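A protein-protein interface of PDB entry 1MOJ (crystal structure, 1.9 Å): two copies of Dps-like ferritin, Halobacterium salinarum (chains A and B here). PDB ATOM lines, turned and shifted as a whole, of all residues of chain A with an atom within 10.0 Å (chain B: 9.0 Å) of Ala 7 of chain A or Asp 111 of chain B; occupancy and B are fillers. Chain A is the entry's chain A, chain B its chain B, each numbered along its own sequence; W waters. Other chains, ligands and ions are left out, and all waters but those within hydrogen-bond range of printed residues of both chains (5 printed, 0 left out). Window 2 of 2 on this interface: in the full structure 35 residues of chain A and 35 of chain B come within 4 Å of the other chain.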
ATOM      1  N   SER A   2       4.646 -14.652 -12.152  1.00  0.00           N
ATOM      2  CA  SER A   2       4.865 -14.624 -10.668  1.00  0.00           C
ATOM      3  C   SER A   2       3.645 -15.130  -9.902  1.00  0.00           C
ATOM      4  O   SER A   2       3.719 -16.106  -9.156  1.00  0.00           O
ATOM      5  CB  SER A   2       5.187 -13.203 -10.211  1.00  0.00           C
ATOM      6  OG  SER A   2       5.330 -13.166  -8.801  1.00  0.00           O
ATOM      7  N   THR A   3       2.530 -14.434 -10.087  1.00  0.00           N
ATOM      8  CA  THR A   3       1.254 -14.770  -9.465  1.00  0.00           C
ATOM      9  C   THR A   3       0.740 -16.036 -10.122  1.00  0.00           C
ATOM     10  O   THR A   3      -0.216 -16.657  -9.655  1.00  0.00           O
ATOM     11  CB  THR A   3       0.225 -13.643  -9.723  1.00  0.00           C
ATOM     12  OG1 THR A   3       0.578 -12.497  -8.946  1.00  0.00           O
ATOM     13  CG2 THR A   3      -1.184 -14.084  -9.368  1.00  0.00           C
ATOM     14  N   GLN A   4       1.412 -16.421 -11.202  1.00  0.00           N
ATOM     15  CA  GLN A   4       1.008 -17.564 -11.999  1.00  0.00           C
ATOM     16  C   GLN A   4       1.933 -18.785 -12.045  1.00  0.00           C
ATOM     17  O   GLN A   4       1.780 -19.648 -12.909  1.00  0.00           O
ATOM     18  CB  GLN A   4       0.720 -17.055 -13.411  1.00  0.00           C
ATOM     19  CG  GLN A   4      -0.205 -15.833 -13.401  1.00  0.00           C
ATOM     20  CD  GLN A   4      -0.147 -15.034 -14.684  1.00  0.00           C
ATOM     21  OE1 GLN A   4       0.889 -14.465 -15.028  1.00  0.00           O
ATOM     22  NE2 GLN A   4      -1.261 -14.988 -15.402  1.00  0.00           N
ATOM     23  N   LYS A   5       2.892 -18.874 -11.131  1.00  0.00           N
ATOM     24  CA  LYS A   5       3.765 -20.044 -11.126  1.00  0.00           C
ATOM     25  C   LYS A   5       2.919 -21.157 -10.516  1.00  0.00           C
ATOM     26  O   LYS A   5       2.039 -20.892  -9.694  1.00  0.00           O
ATOM     27  CB  LYS A   5       4.999 -19.808 -10.257  1.00  0.00           C
ATOM     28  CG  LYS A   5       5.778 -18.546 -10.580  1.00  0.00           C
ATOM     29  CD  LYS A   5       7.056 -18.486  -9.749  1.00  0.00           C
ATOM     30  CE  LYS A   5       6.772 -18.697  -8.270  1.00  0.00           C
ATOM     31  NZ  LYS A   5       8.005 -18.699  -7.435  1.00  0.00           N
ATOM     32  N   ASN A   6       3.155 -22.397 -10.918  1.00  0.00           N
ATOM     33  CA  ASN A   6       2.370 -23.488 -10.359  1.00  0.00           C
ATOM     34  C   ASN A   6       2.868 -23.796  -8.956  1.00  0.00           C
ATOM     35  O   ASN A   6       2.088 -23.903  -8.005  1.00  0.00           O
ATOM     36  CB  ASN A   6       2.471 -24.733 -11.244  1.00  0.00           C
ATOM     37  CG  ASN A   6       1.752 -24.562 -12.571  1.00  0.00           C
ATOM     38  OD1 ASN A   6       0.590 -24.153 -12.607  1.00  0.00           O
ATOM     39  ND2 ASN A   6       2.434 -24.879 -13.667  1.00  0.00           N
ATOM     40  N   ALA A   7       4.183 -23.909  -8.832  1.00  0.00           N
ATOM     41  CA  ALA A   7       4.809 -24.210  -7.557  1.00  0.00           C
ATOM     42  C   ALA A   7       4.425 -23.212  -6.478  1.00  0.00           C
ATOM     43  O   ALA A   7       4.413 -21.996  -6.696  1.00  0.00           O
ATOM     44  CB  ALA A   7       6.332 -24.248  -7.716  1.00  0.00           C
ATOM     45  N   ARG A   8       4.083 -23.745  -5.315  1.00  0.00           N
ATOM     46  CA  ARG A   8       3.741 -22.918  -4.180  1.00  0.00           C
ATOM     47  C   ARG A   8       5.046 -22.355  -3.619  1.00  0.00           C
ATOM     48  O   ARG A   8       5.073 -21.250  -3.078  1.00  0.00           O
ATOM     49  CB  ARG A   8       3.021 -23.760  -3.133  1.00  0.00           C
ATOM     50  CG  ARG A   8       2.486 -22.941  -2.011  1.00  0.00           C
ATOM     51  CD  ARG A   8       1.590 -23.738  -1.089  1.00  0.00           C
ATOM     52  NE  ARG A   8       1.256 -22.930   0.082  1.00  0.00           N
ATOM     53  CZ  ARG A   8       0.509 -21.833   0.045  1.00  0.00           C
ATOM     54  NH1 ARG A   8       0.001 -21.406  -1.106  1.00  0.00           N
ATOM     55  NH2 ARG A   8       0.291 -21.148   1.161  1.00  0.00           N
ATOM     56  N   ALA A   9       6.123 -23.129  -3.749  1.00  0.00           N
ATOM     57  CA  ALA A   9       7.449 -22.731  -3.294  1.00  0.00           C
ATOM     58  C   ALA A   9       8.473 -23.384  -4.204  1.00  0.00           C
ATOM     59  O   ALA A   9       8.263 -24.501  -4.677  1.00  0.00           O
ATOM     60  CB  ALA A   9       7.679 -23.171  -1.844  1.00  0.00           C
ATOM     61  N   THR A  10       9.576 -22.686  -4.453  1.00  0.00           N
ATOM     62  CA  THR A  10      10.633 -23.201  -5.317  1.00  0.00           C
ATOM     63  C   THR A  10      11.824 -23.690  -4.504  1.00  0.00           C
ATOM     64  O   THR A  10      12.315 -22.984  -3.635  1.00  0.00           O
ATOM     65  CB  THR A  10      11.118 -22.110  -6.315  1.00  0.00           C
ATOM     66  OG1 THR A  10      10.075 -21.828  -7.255  1.00  0.00           O
ATOM     67  CG2 THR A  10      12.357 -22.572  -7.071  1.00  0.00           C
ATOM     68  N   ALA A  11      12.281 -24.901  -4.795  1.00  0.00           N
ATOM     69  CA  ALA A  11      13.416 -25.467  -4.085  1.00  0.00           C
ATOM     70  C   ALA A  11      14.587 -24.492  -4.143  1.00  0.00           C
ATOM     71  O   ALA A  11      14.868 -23.920  -5.196  1.00  0.00           O
ATOM     72  CB  ALA A  11      13.810 -26.793  -4.713  1.00  0.00           C
ATOM     73  N   GLY A  12      15.262 -24.296  -3.014  1.00  0.00           N
ATOM     74  CA  GLY A  12      16.398 -23.387  -2.984  1.00  0.00           C
ATOM     75  C   GLY A  12      16.081 -21.995  -2.460  1.00  0.00           C
ATOM     76  O   GLY A  12      16.977 -21.246  -2.049  1.00  0.00           O
ATOM     77  N   GLU A  13      14.806 -21.635  -2.467  1.00  0.00           N
ATOM     78  CA  GLU A  13      14.397 -20.321  -1.986  1.00  0.00           C
ATOM     79  C   GLU A  13      14.142 -20.310  -0.480  1.00  0.00           C
ATOM     80  O   GLU A  13      13.669 -21.298   0.090  1.00  0.00           O
ATOM     81  CB  GLU A  13      13.138 -19.863  -2.725  1.00  0.00           C
ATOM     82  CG  GLU A  13      13.351 -19.623  -4.219  1.00  0.00           C
ATOM     83  CD  GLU A  13      12.055 -19.305  -4.954  1.00  0.00           C
ATOM     84  OE1 GLU A  13      12.119 -19.014  -6.167  1.00  0.00           O
ATOM     85  OE2 GLU A  13      10.971 -19.350  -4.324  1.00  0.00           O
ATOM     86  N   GLY A  90      12.137 -21.957   4.191  1.00  0.00           N
ATOM     87  CA  GLY A  90      12.883 -22.689   3.186  1.00  0.00           C
ATOM     88  C   GLY A  90      12.188 -23.955   2.696  1.00  0.00           C
ATOM     89  O   GLY A  90      11.067 -24.279   3.117  1.00  0.00           O
ATOM     90  N   VAL A  91      12.852 -24.668   1.790  1.00  0.00           N
ATOM     91  CA  VAL A  91      12.320 -25.916   1.238  1.00  0.00           C
ATOM     92  C   VAL A  91      13.251 -27.068   1.607  1.00  0.00           C
ATOM     93  O   VAL A  91      14.372 -27.175   1.104  1.00  0.00           O
ATOM     94  CB  VAL A  91      12.191 -25.862  -0.306  1.00  0.00           C
ATOM     95  CG1 VAL A  91      11.724 -27.203  -0.839  1.00  0.00           C
ATOM     96  CG2 VAL A  91      11.206 -24.777  -0.709  1.00  0.00           C
ATOM     97  N   PRO A  92      12.795 -27.943   2.507  1.00  0.00           N
ATOM     98  CA  PRO A  92      13.634 -29.078   2.905  1.00  0.00           C
ATOM     99  C   PRO A  92      13.795 -30.103   1.785  1.00  0.00           C
ATOM    100  O   PRO A  92      12.843 -30.380   1.041  1.00  0.00           O
ATOM    101  CB  PRO A  92      12.894 -29.642   4.118  1.00  0.00           C
ATOM    102  CG  PRO A  92      11.454 -29.327   3.801  1.00  0.00           C
ATOM    103  CD  PRO A  92      11.536 -27.911   3.275  1.00  0.00           C
ATOM    104  N   HIS A  93      15.008 -30.640   1.649  1.00  0.00           N
ATOM    105  CA  HIS A  93      15.278 -31.661   0.634  1.00  0.00           C
ATOM    106  C   HIS A  93      14.299 -32.772   0.941  1.00  0.00           C
ATOM    107  O   HIS A  93      14.162 -33.184   2.098  1.00  0.00           O
ATOM    108  CB  HIS A  93      16.716 -32.172   0.746  1.00  0.00           C
ATOM    109  CG  HIS A  93      17.745 -31.114   0.510  1.00  0.00           C
ATOM    110  ND1 HIS A  93      17.695 -30.257  -0.570  1.00  0.00           N
ATOM    111  CD2 HIS A  93      18.847 -30.767   1.214  1.00  0.00           C
ATOM    112  CE1 HIS A  93      18.719 -29.425  -0.518  1.00  0.00           C
ATOM    113  NE2 HIS A  93      19.435 -29.711   0.555  1.00  0.00           N
ATOM    114  N   ALA A  94      13.616 -33.260  -0.079  1.00  0.00           N
ATOM    115  CA  ALA A  94      12.616 -34.282   0.158  1.00  0.00           C
ATOM    116  C   ALA A  94      12.825 -35.635  -0.505  1.00  0.00           C
ATOM    117  O   ALA A  94      12.876 -36.648   0.179  1.00  0.00           O
ATOM    118  CB  ALA A  94      11.244 -33.722  -0.218  1.00  0.00           C
ATOM    119  N   SER A  95      12.929 -35.667  -1.831  1.00  0.00           N
ATOM    120  CA  SER A  95      13.077 -36.942  -2.518  1.00  0.00           C
ATOM    121  C   SER A  95      14.350 -37.663  -2.107  1.00  0.00           C
ATOM    122  O   SER A  95      15.342 -37.035  -1.732  1.00  0.00           O
ATOM    123  CB  SER A  95      13.047 -36.771  -4.050  1.00  0.00           C
ATOM    124  OG  SER A  95      14.250 -36.219  -4.553  1.00  0.00           O
ATOM    125  N   THR A  98      17.276 -36.565  -4.082  1.00  0.00           N
ATOM    126  CA  THR A  98      17.767 -35.251  -3.671  1.00  0.00           C
ATOM    127  C   THR A  98      18.552 -35.335  -2.363  1.00  0.00           C
ATOM    128  O   THR A  98      19.607 -34.710  -2.206  1.00  0.00           O
ATOM    129  CB  THR A  98      16.618 -34.249  -3.440  1.00  0.00           C
ATOM    130  OG1 THR A  98      15.875 -34.081  -4.650  1.00  0.00           O
ATOM    131  CG2 THR A  98      17.175 -32.895  -2.998  1.00  0.00           C
ATOM    132  N   GLN B  47       7.733 -38.737   0.270  1.00  0.00           N
ATOM    133  CA  GLN B  47       6.862 -37.712  -0.287  1.00  0.00           C
ATOM    134  C   GLN B  47       5.794 -37.336   0.742  1.00  0.00           C
ATOM    135  O   GLN B  47       5.377 -36.184   0.820  1.00  0.00           O
ATOM    136  CB  GLN B  47       6.216 -38.189  -1.596  1.00  0.00           C
ATOM    137  CG  GLN B  47       5.481 -37.057  -2.327  1.00  0.00           C
ATOM    138  CD  GLN B  47       5.479 -37.223  -3.841  1.00  0.00           C
ATOM    139  OE1 GLN B  47       6.525 -37.125  -4.492  1.00  0.00           O
ATOM    140  NE2 GLN B  47       4.304 -37.478  -4.407  1.00  0.00           N
ATOM    141  N   LYS B  50       7.445 -35.024   2.976  1.00  0.00           N
ATOM    142  CA  LYS B  50       7.529 -33.728   2.312  1.00  0.00           C
ATOM    143  C   LYS B  50       6.250 -32.922   2.476  1.00  0.00           C
ATOM    144  O   LYS B  50       6.286 -31.759   2.856  1.00  0.00           O
ATOM    145  CB  LYS B  50       7.800 -33.902   0.822  1.00  0.00           C
ATOM    146  CG  LYS B  50       7.802 -32.591   0.047  1.00  0.00           C
ATOM    147  CD  LYS B  50       7.881 -32.848  -1.456  1.00  0.00           C
ATOM    148  CE  LYS B  50       8.045 -31.556  -2.268  1.00  0.00           C
ATOM    149  NZ  LYS B  50       8.126 -31.854  -3.733  1.00  0.00           N
ATOM    150  N   HIS B  51       5.117 -33.543   2.184  1.00  0.00           N
ATOM    151  CA  HIS B  51       3.834 -32.857   2.291  1.00  0.00           C
ATOM    152  C   HIS B  51       3.472 -32.551   3.740  1.00  0.00           C
ATOM    153  O   HIS B  51       2.853 -31.529   4.042  1.00  0.00           O
ATOM    154  CB  HIS B  51       2.776 -33.703   1.589  1.00  0.00           C
ATOM    155  CG  HIS B  51       3.053 -33.883   0.127  1.00  0.00           C
ATOM    156  ND1 HIS B  51       2.479 -34.880  -0.634  1.00  0.00           N
ATOM    157  CD2 HIS B  51       3.863 -33.190  -0.712  1.00  0.00           C
ATOM    158  CE1 HIS B  51       2.924 -34.797  -1.876  1.00  0.00           C
ATOM    159  NE2 HIS B  51       3.765 -33.779  -1.951  1.00  0.00           N
ATOM    160  N   ASN B  54       5.576 -29.445   4.583  1.00  0.00           N
ATOM    161  CA  ASN B  54       5.148 -28.261   3.851  1.00  0.00           C
ATOM    162  C   ASN B  54       3.687 -27.829   3.841  1.00  0.00           C
ATOM    163  O   ASN B  54       3.396 -26.679   3.500  1.00  0.00           O
ATOM    164  CB  ASN B  54       5.616 -28.385   2.399  1.00  0.00           C
ATOM    165  CG  ASN B  54       7.128 -28.439   2.273  1.00  0.00           C
ATOM    166  OD1 ASN B  54       7.826 -27.548   2.744  1.00  0.00           O
ATOM    167  ND2 ASN B  54       7.640 -29.484   1.626  1.00  0.00           N
ATOM    168  N   VAL B 107       7.679 -39.366  -8.641  1.00  0.00           N
ATOM    169  CA  VAL B 107       7.993 -38.548  -7.473  1.00  0.00           C
ATOM    170  C   VAL B 107       8.033 -37.084  -7.895  1.00  0.00           C
ATOM    171  O   VAL B 107       8.574 -36.745  -8.949  1.00  0.00           O
ATOM    172  CB  VAL B 107       9.364 -38.933  -6.837  1.00  0.00           C
ATOM    173  CG1 VAL B 107       9.557 -40.429  -6.891  1.00  0.00           C
ATOM    174  CG2 VAL B 107      10.501 -38.214  -7.531  1.00  0.00           C
ATOM    175  N   GLU B 108       7.447 -36.219  -7.079  1.00  0.00           N
ATOM    176  CA  GLU B 108       7.442 -34.795  -7.372  1.00  0.00           C
ATOM    177  C   GLU B 108       8.861 -34.277  -7.436  1.00  0.00           C
ATOM    178  O   GLU B 108       9.760 -34.853  -6.826  1.00  0.00           O
ATOM    179  CB  GLU B 108       6.729 -34.019  -6.274  1.00  0.00           C
ATOM    180  CG  GLU B 108       5.238 -34.162  -6.244  1.00  0.00           C
ATOM    181  CD  GLU B 108       4.632 -33.403  -5.082  1.00  0.00           C
ATOM    182  OE1 GLU B 108       3.398 -33.455  -4.922  1.00  0.00           O
ATOM    183  OE2 GLU B 108       5.390 -32.760  -4.330  1.00  0.00           O
ATOM    184  N   ASP B 109       9.071 -33.187  -8.165  1.00  0.00           N
ATOM    185  CA  ASP B 109      10.397 -32.603  -8.210  1.00  0.00           C
ATOM    186  C   ASP B 109      10.519 -31.863  -6.879  1.00  0.00           C
ATOM    187  O   ASP B 109       9.582 -31.876  -6.085  1.00  0.00           O
ATOM    188  CB  ASP B 109      10.560 -31.664  -9.418  1.00  0.00           C
ATOM    189  CG  ASP B 109       9.582 -30.506  -9.418  1.00  0.00           C
ATOM    190  OD1 ASP B 109       9.254 -30.033 -10.524  1.00  0.00           O
ATOM    191  OD2 ASP B 109       9.154 -30.057  -8.337  1.00  0.00           O
ATOM    192  N   GLU B 110      11.652 -31.218  -6.633  1.00  0.00           N
ATOM    193  CA  GLU B 110      11.864 -30.544  -5.356  1.00  0.00           C
ATOM    194  C   GLU B 110      11.061 -29.303  -5.011  1.00  0.00           C
ATOM    195  O   GLU B 110      11.173 -28.786  -3.901  1.00  0.00           O
ATOM    196  CB  GLU B 110      13.356 -30.277  -5.157  1.00  0.00           C
ATOM    197  CG  GLU B 110      14.119 -31.554  -4.818  1.00  0.00           C
ATOM    198  CD  GLU B 110      13.547 -32.279  -3.596  1.00  0.00           C
ATOM    199  OE1 GLU B 110      12.875 -33.326  -3.764  1.00  0.00           O
ATOM    200  OE2 GLU B 110      13.762 -31.783  -2.468  1.00  0.00           O
ATOM    201  N   ASP B 111      10.245 -28.818  -5.938  1.00  0.00           N
ATOM    202  CA  ASP B 111       9.430 -27.653  -5.625  1.00  0.00           C
ATOM    203  C   ASP B 111       8.256 -28.117  -4.765  1.00  0.00           C
ATOM    204  O   ASP B 111       7.941 -29.305  -4.724  1.00  0.00           O
ATOM    205  CB  ASP B 111       8.906 -26.976  -6.897  1.00  0.00           C
ATOM    206  CG  ASP B 111      10.008 -26.311  -7.693  1.00  0.00           C
ATOM    207  OD1 ASP B 111      11.057 -25.966  -7.110  1.00  0.00           O
ATOM    208  OD2 ASP B 111       9.817 -26.123  -8.911  1.00  0.00           O
ATOM    209  N   VAL B 112       7.628 -27.169  -4.080  1.00  0.00           N
ATOM    210  CA  VAL B 112       6.490 -27.453  -3.215  1.00  0.00           C
ATOM    211  C   VAL B 112       5.223 -27.010  -3.923  1.00  0.00           C
ATOM    212  O   VAL B 112       5.117 -25.858  -4.357  1.00  0.00           O
ATOM    213  CB  VAL B 112       6.608 -26.686  -1.874  1.00  0.00           C
ATOM    214  CG1 VAL B 112       5.369 -26.934  -1.011  1.00  0.00           C
ATOM    215  CG2 VAL B 112       7.873 -27.115  -1.141  1.00  0.00           C
ATOM    216  N   TYR B 113       4.262 -27.914  -4.042  1.00  0.00           N
ATOM    217  CA  TYR B 113       3.008 -27.594  -4.707  1.00  0.00           C
ATOM    218  C   TYR B 113       1.891 -27.373  -3.697  1.00  0.00           C
ATOM    219  O   TYR B 113       2.068 -27.667  -2.505  1.00  0.00           O
ATOM    220  CB  TYR B 113       2.652 -28.712  -5.689  1.00  0.00           C
ATOM    221  CG  TYR B 113       3.733 -28.900  -6.725  1.00  0.00           C
ATOM    222  CD1 TYR B 113       4.673 -29.920  -6.608  1.00  0.00           C
ATOM    223  CD2 TYR B 113       3.883 -27.983  -7.769  1.00  0.00           C
ATOM    224  CE1 TYR B 113       5.744 -30.021  -7.503  1.00  0.00           C
ATOM    225  CE2 TYR B 113       4.947 -28.069  -8.660  1.00  0.00           C
ATOM    226  CZ  TYR B 113       5.873 -29.088  -8.521  1.00  0.00           C
ATOM    227  OH  TYR B 113       6.934 -29.157  -9.394  1.00  0.00           O
ATOM    228  N   ASP B 114       0.759 -26.834  -4.157  1.00  0.00           N
ATOM    229  CA  ASP B 114      -0.358 -26.595  -3.250  1.00  0.00           C
ATOM    230  C   ASP B 114      -0.838 -27.943  -2.735  1.00  0.00           C
ATOM    231  O   ASP B 114      -0.576 -28.974  -3.354  1.00  0.00           O
ATOM    232  CB  ASP B 114      -1.482 -25.802  -3.932  1.00  0.00           C
ATOM    233  CG  ASP B 114      -2.144 -26.545  -5.068  1.00  0.00           C
ATOM    234  OD1 ASP B 114      -2.571 -25.871  -6.029  1.00  0.00           O
ATOM    235  OD2 ASP B 114      -2.268 -27.781  -5.011  1.00  0.00           O
ATOM    236  N   THR B 117      -2.741 -30.485  -5.115  1.00  0.00           N
ATOM    237  CA  THR B 117      -1.842 -31.096  -6.095  1.00  0.00           C
ATOM    238  C   THR B 117      -0.971 -32.147  -5.411  1.00  0.00           C
ATOM    239  O   THR B 117      -0.812 -33.249  -5.912  1.00  0.00           O
ATOM    240  CB  THR B 117      -0.906 -30.043  -6.749  1.00  0.00           C
ATOM    241  OG1 THR B 117      -1.691 -29.120  -7.515  1.00  0.00           O
ATOM    242  CG2 THR B 117       0.120 -30.725  -7.662  1.00  0.00           C
ATOM    243  N   SER B 118      -0.415 -31.783  -4.263  1.00  0.00           N
ATOM    244  CA  SER B 118       0.446 -32.678  -3.493  1.00  0.00           C
ATOM    245  C   SER B 118      -0.287 -33.980  -3.160  1.00  0.00           C
ATOM    246  O   SER B 118       0.211 -35.073  -3.417  1.00  0.00           O
ATOM    247  CB  SER B 118       0.873 -31.986  -2.192  1.00  0.00           C
ATOM    248  OG  SER B 118       1.542 -30.763  -2.453  1.00  0.00           O
ATOM    249  N   ASN B 121      -0.952 -36.241  -6.072  1.00  0.00           N
ATOM    250  CA  ASN B 121       0.242 -36.979  -6.465  1.00  0.00           C
ATOM    251  C   ASN B 121       0.417 -38.201  -5.566  1.00  0.00           C
ATOM    252  O   ASN B 121       0.738 -39.291  -6.044  1.00  0.00           O
ATOM    253  CB  ASN B 121       1.491 -36.090  -6.385  1.00  0.00           C
ATOM    254  CG  ASN B 121       1.532 -35.058  -7.493  1.00  0.00           C
ATOM    255  OD1 ASN B 121       0.987 -35.291  -8.574  1.00  0.00           O
ATOM    256  ND2 ASN B 121       2.186 -33.916  -7.243  1.00  0.00           N
HETATM  257  O   HOH W   1      15.702 -29.611  -2.190  1.00  0.00           O
HETATM  258  O   HOH W   2      10.240 -30.057   0.571  1.00  0.00           O
HETATM  259  O   HOH W   3       2.995 -25.205   1.266  1.00  0.00           O
HETATM  260  O   HOH W   4      10.979 -30.445  -1.859  1.00  0.00           O
HETATM  261  O   HOH W   5       0.818 -25.574  -6.681  1.00  0.00           O
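Of the 19 printed residues of chain A, 11 touch a printed residue of chain B.
Hydrophobic or aromatic side chains of chain A that line the printed part of chain B: Ala 7, Ala 9, Ala 11, Val 91, Pro 92 and Ala 94.
Of the 15 printed residues of chain B, 7 touch a printed residue of chain A.
Printed residues of chain B that touch a printed residue of chain A: Lys 50, Asn 54, Glu 110, Asp 111, Val 112, Tyr 113 and Asp 114.
Among the printed residues, 20 pairs touch across the chains.
The side-chain amide nitrogen (ND2) of Asn 54 of chain B sits at hydrogen-bond distance from the backbone carbonyl oxygen (O) of Lys 50 of chain B.
The side-chain carboxylate (OE2) of Glu 108 of chain B lies within salt-bridge range of the side-chain amino group (NZ) of Lys 50 of chain B (2.9 Å).
The backbone carbonyl oxygen (O) of Asp 109 of chain B lies within hydrogen-bond range of the side-chain amino group (NZ) of Lys 50 of chain B, at 2.8 Å.
NZ of Lys 50 of chain B lies within hydrogen-bond range of O of Asp 111 of chain B.
The side-chain hydroxyl (OG) of Ser 118 of chain B lies within hydrogen-bond range of the backbone carbonyl oxygen (O) of Tyr 113 of chain B (3.1 Å).
The backbone carbonyl oxygen of Asp 114 of chain B is in hydrogen-bond range of the side-chain hydroxyl of Ser 118 of chain B.
O of Val 112 of chain B lies within hydrogen-bond range of N of Arg 8 of chain A.
The backbone NH (N) of Val 112 of chain B sits at hydrogen-bond distance from the backbone carbonyl oxygen (O) of Ala 9 of chain A, 2.8 Å away.
OD1 of Asp 111 of chain B is in hydrogen-bond range of N of Ala 11 of chain A (2.8 Å).
The backbone NH (N) of Ala 94 of chain A is in hydrogen-bond range of the side-chain carboxylate (OE2) of Glu 110 of chain B (2.8 Å).
The backbone NH (N) of Ser 95 of chain A lies within hydrogen-bond range of the side-chain carboxylate (OE1) of Glu 110 of chain B (3.0 Å).
The side-chain carboxylate (OE1) of Glu 110 of chain B lies close to the side-chain hydroxyl (OG1) of Thr 98 of chain A, 3.2 Å away.
Water W5 bridges O of Asn 6 of chain A (2.5 Å) and N of Asp 114 of chain B (2.8 Å).
Water W4 lies within hydrogen-bond range of the backbone carbonyl oxygen (O) of Glu 110 of chain B and the backbone carbonyl oxygen (O) of Pro 92 of chain A.
Water W1 lies within hydrogen-bond range of ND1 of His 93 of chain A (2.6 Å) and OE2 of Glu 110 of chain B (2.9 Å).
Water W2 lies within hydrogen-bond range of O of Pro 92 of chain A (2.7 Å) and ND2 of Asn 54 of chain B (2.9 Å).
Water W3 lies within hydrogen-bond range of O of Asn 54 of chain B and NE of Arg 8 of chain A.
CB of Asp 111 of chain B touches CB of Ala 7 of chain A, at 3.8 Å.
C of Ala 7 of chain A touches O of Val 112 of chain B (3.5 Å).
Ala 7 of chain A touches Tyr 113 of chain B (CA to CD2, 3.9 Å).
CB of Arg 8 of chain A touches N of Asp 114 of chain B, 3.95 Å away.
Ala 9 of chain A touches Asp 111 of chain B (O to CB, 3.4 Å).
Ala 11 of chain A touches Glu 110 of chain B (CB to O, 3.4 Å).
Glu 110 of chain B touches Val 91 of chain A (O to CG1, 3.5 Å).
Val 91 of chain A touches Val 112 of chain B (CG1 to CG2, 3.9 Å).
Asn 54 of chain B touches Pro 92 of chain A (OD1 to CD, 3.8 Å).
CA of His 93 of chain A touches OE2 of Glu 110 of chain B (3.5 Å).
No position is printed for both chains.
Of the 20 pairs that touch across the chains among the printed residues, none has its exchanged pair printed and touching as well.
Of chain B, only Asp 111 (3.8 Å), Val 112 (3.5 Å) and Tyr 113 (3.9 Å) come within 4 Å of Ala 7 of chain A.
Ala 11 of chain A touches two residues of chain B.
Gly 12 of chain A touches none of the printed residues of chain B.
Printed residues of chain B within 4 Å of Ala 94 of chain A: Lys 50 (3.6 Å) and Glu 110 (2.8 Å).
Of the printed residues of chain B, Thr 98 of chain A touches Glu 110 (3.1 Å).
Gln 47 of chain B touches none of the printed residues of chain A.
Of chain A, only Ala 11, Val 91, Pro 92, His 93, Ala 94, Ser 95 and Thr 98 come within 4 Å of Glu 110 of chain B.
Asp 111 of chain B touches four residues of chain A.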
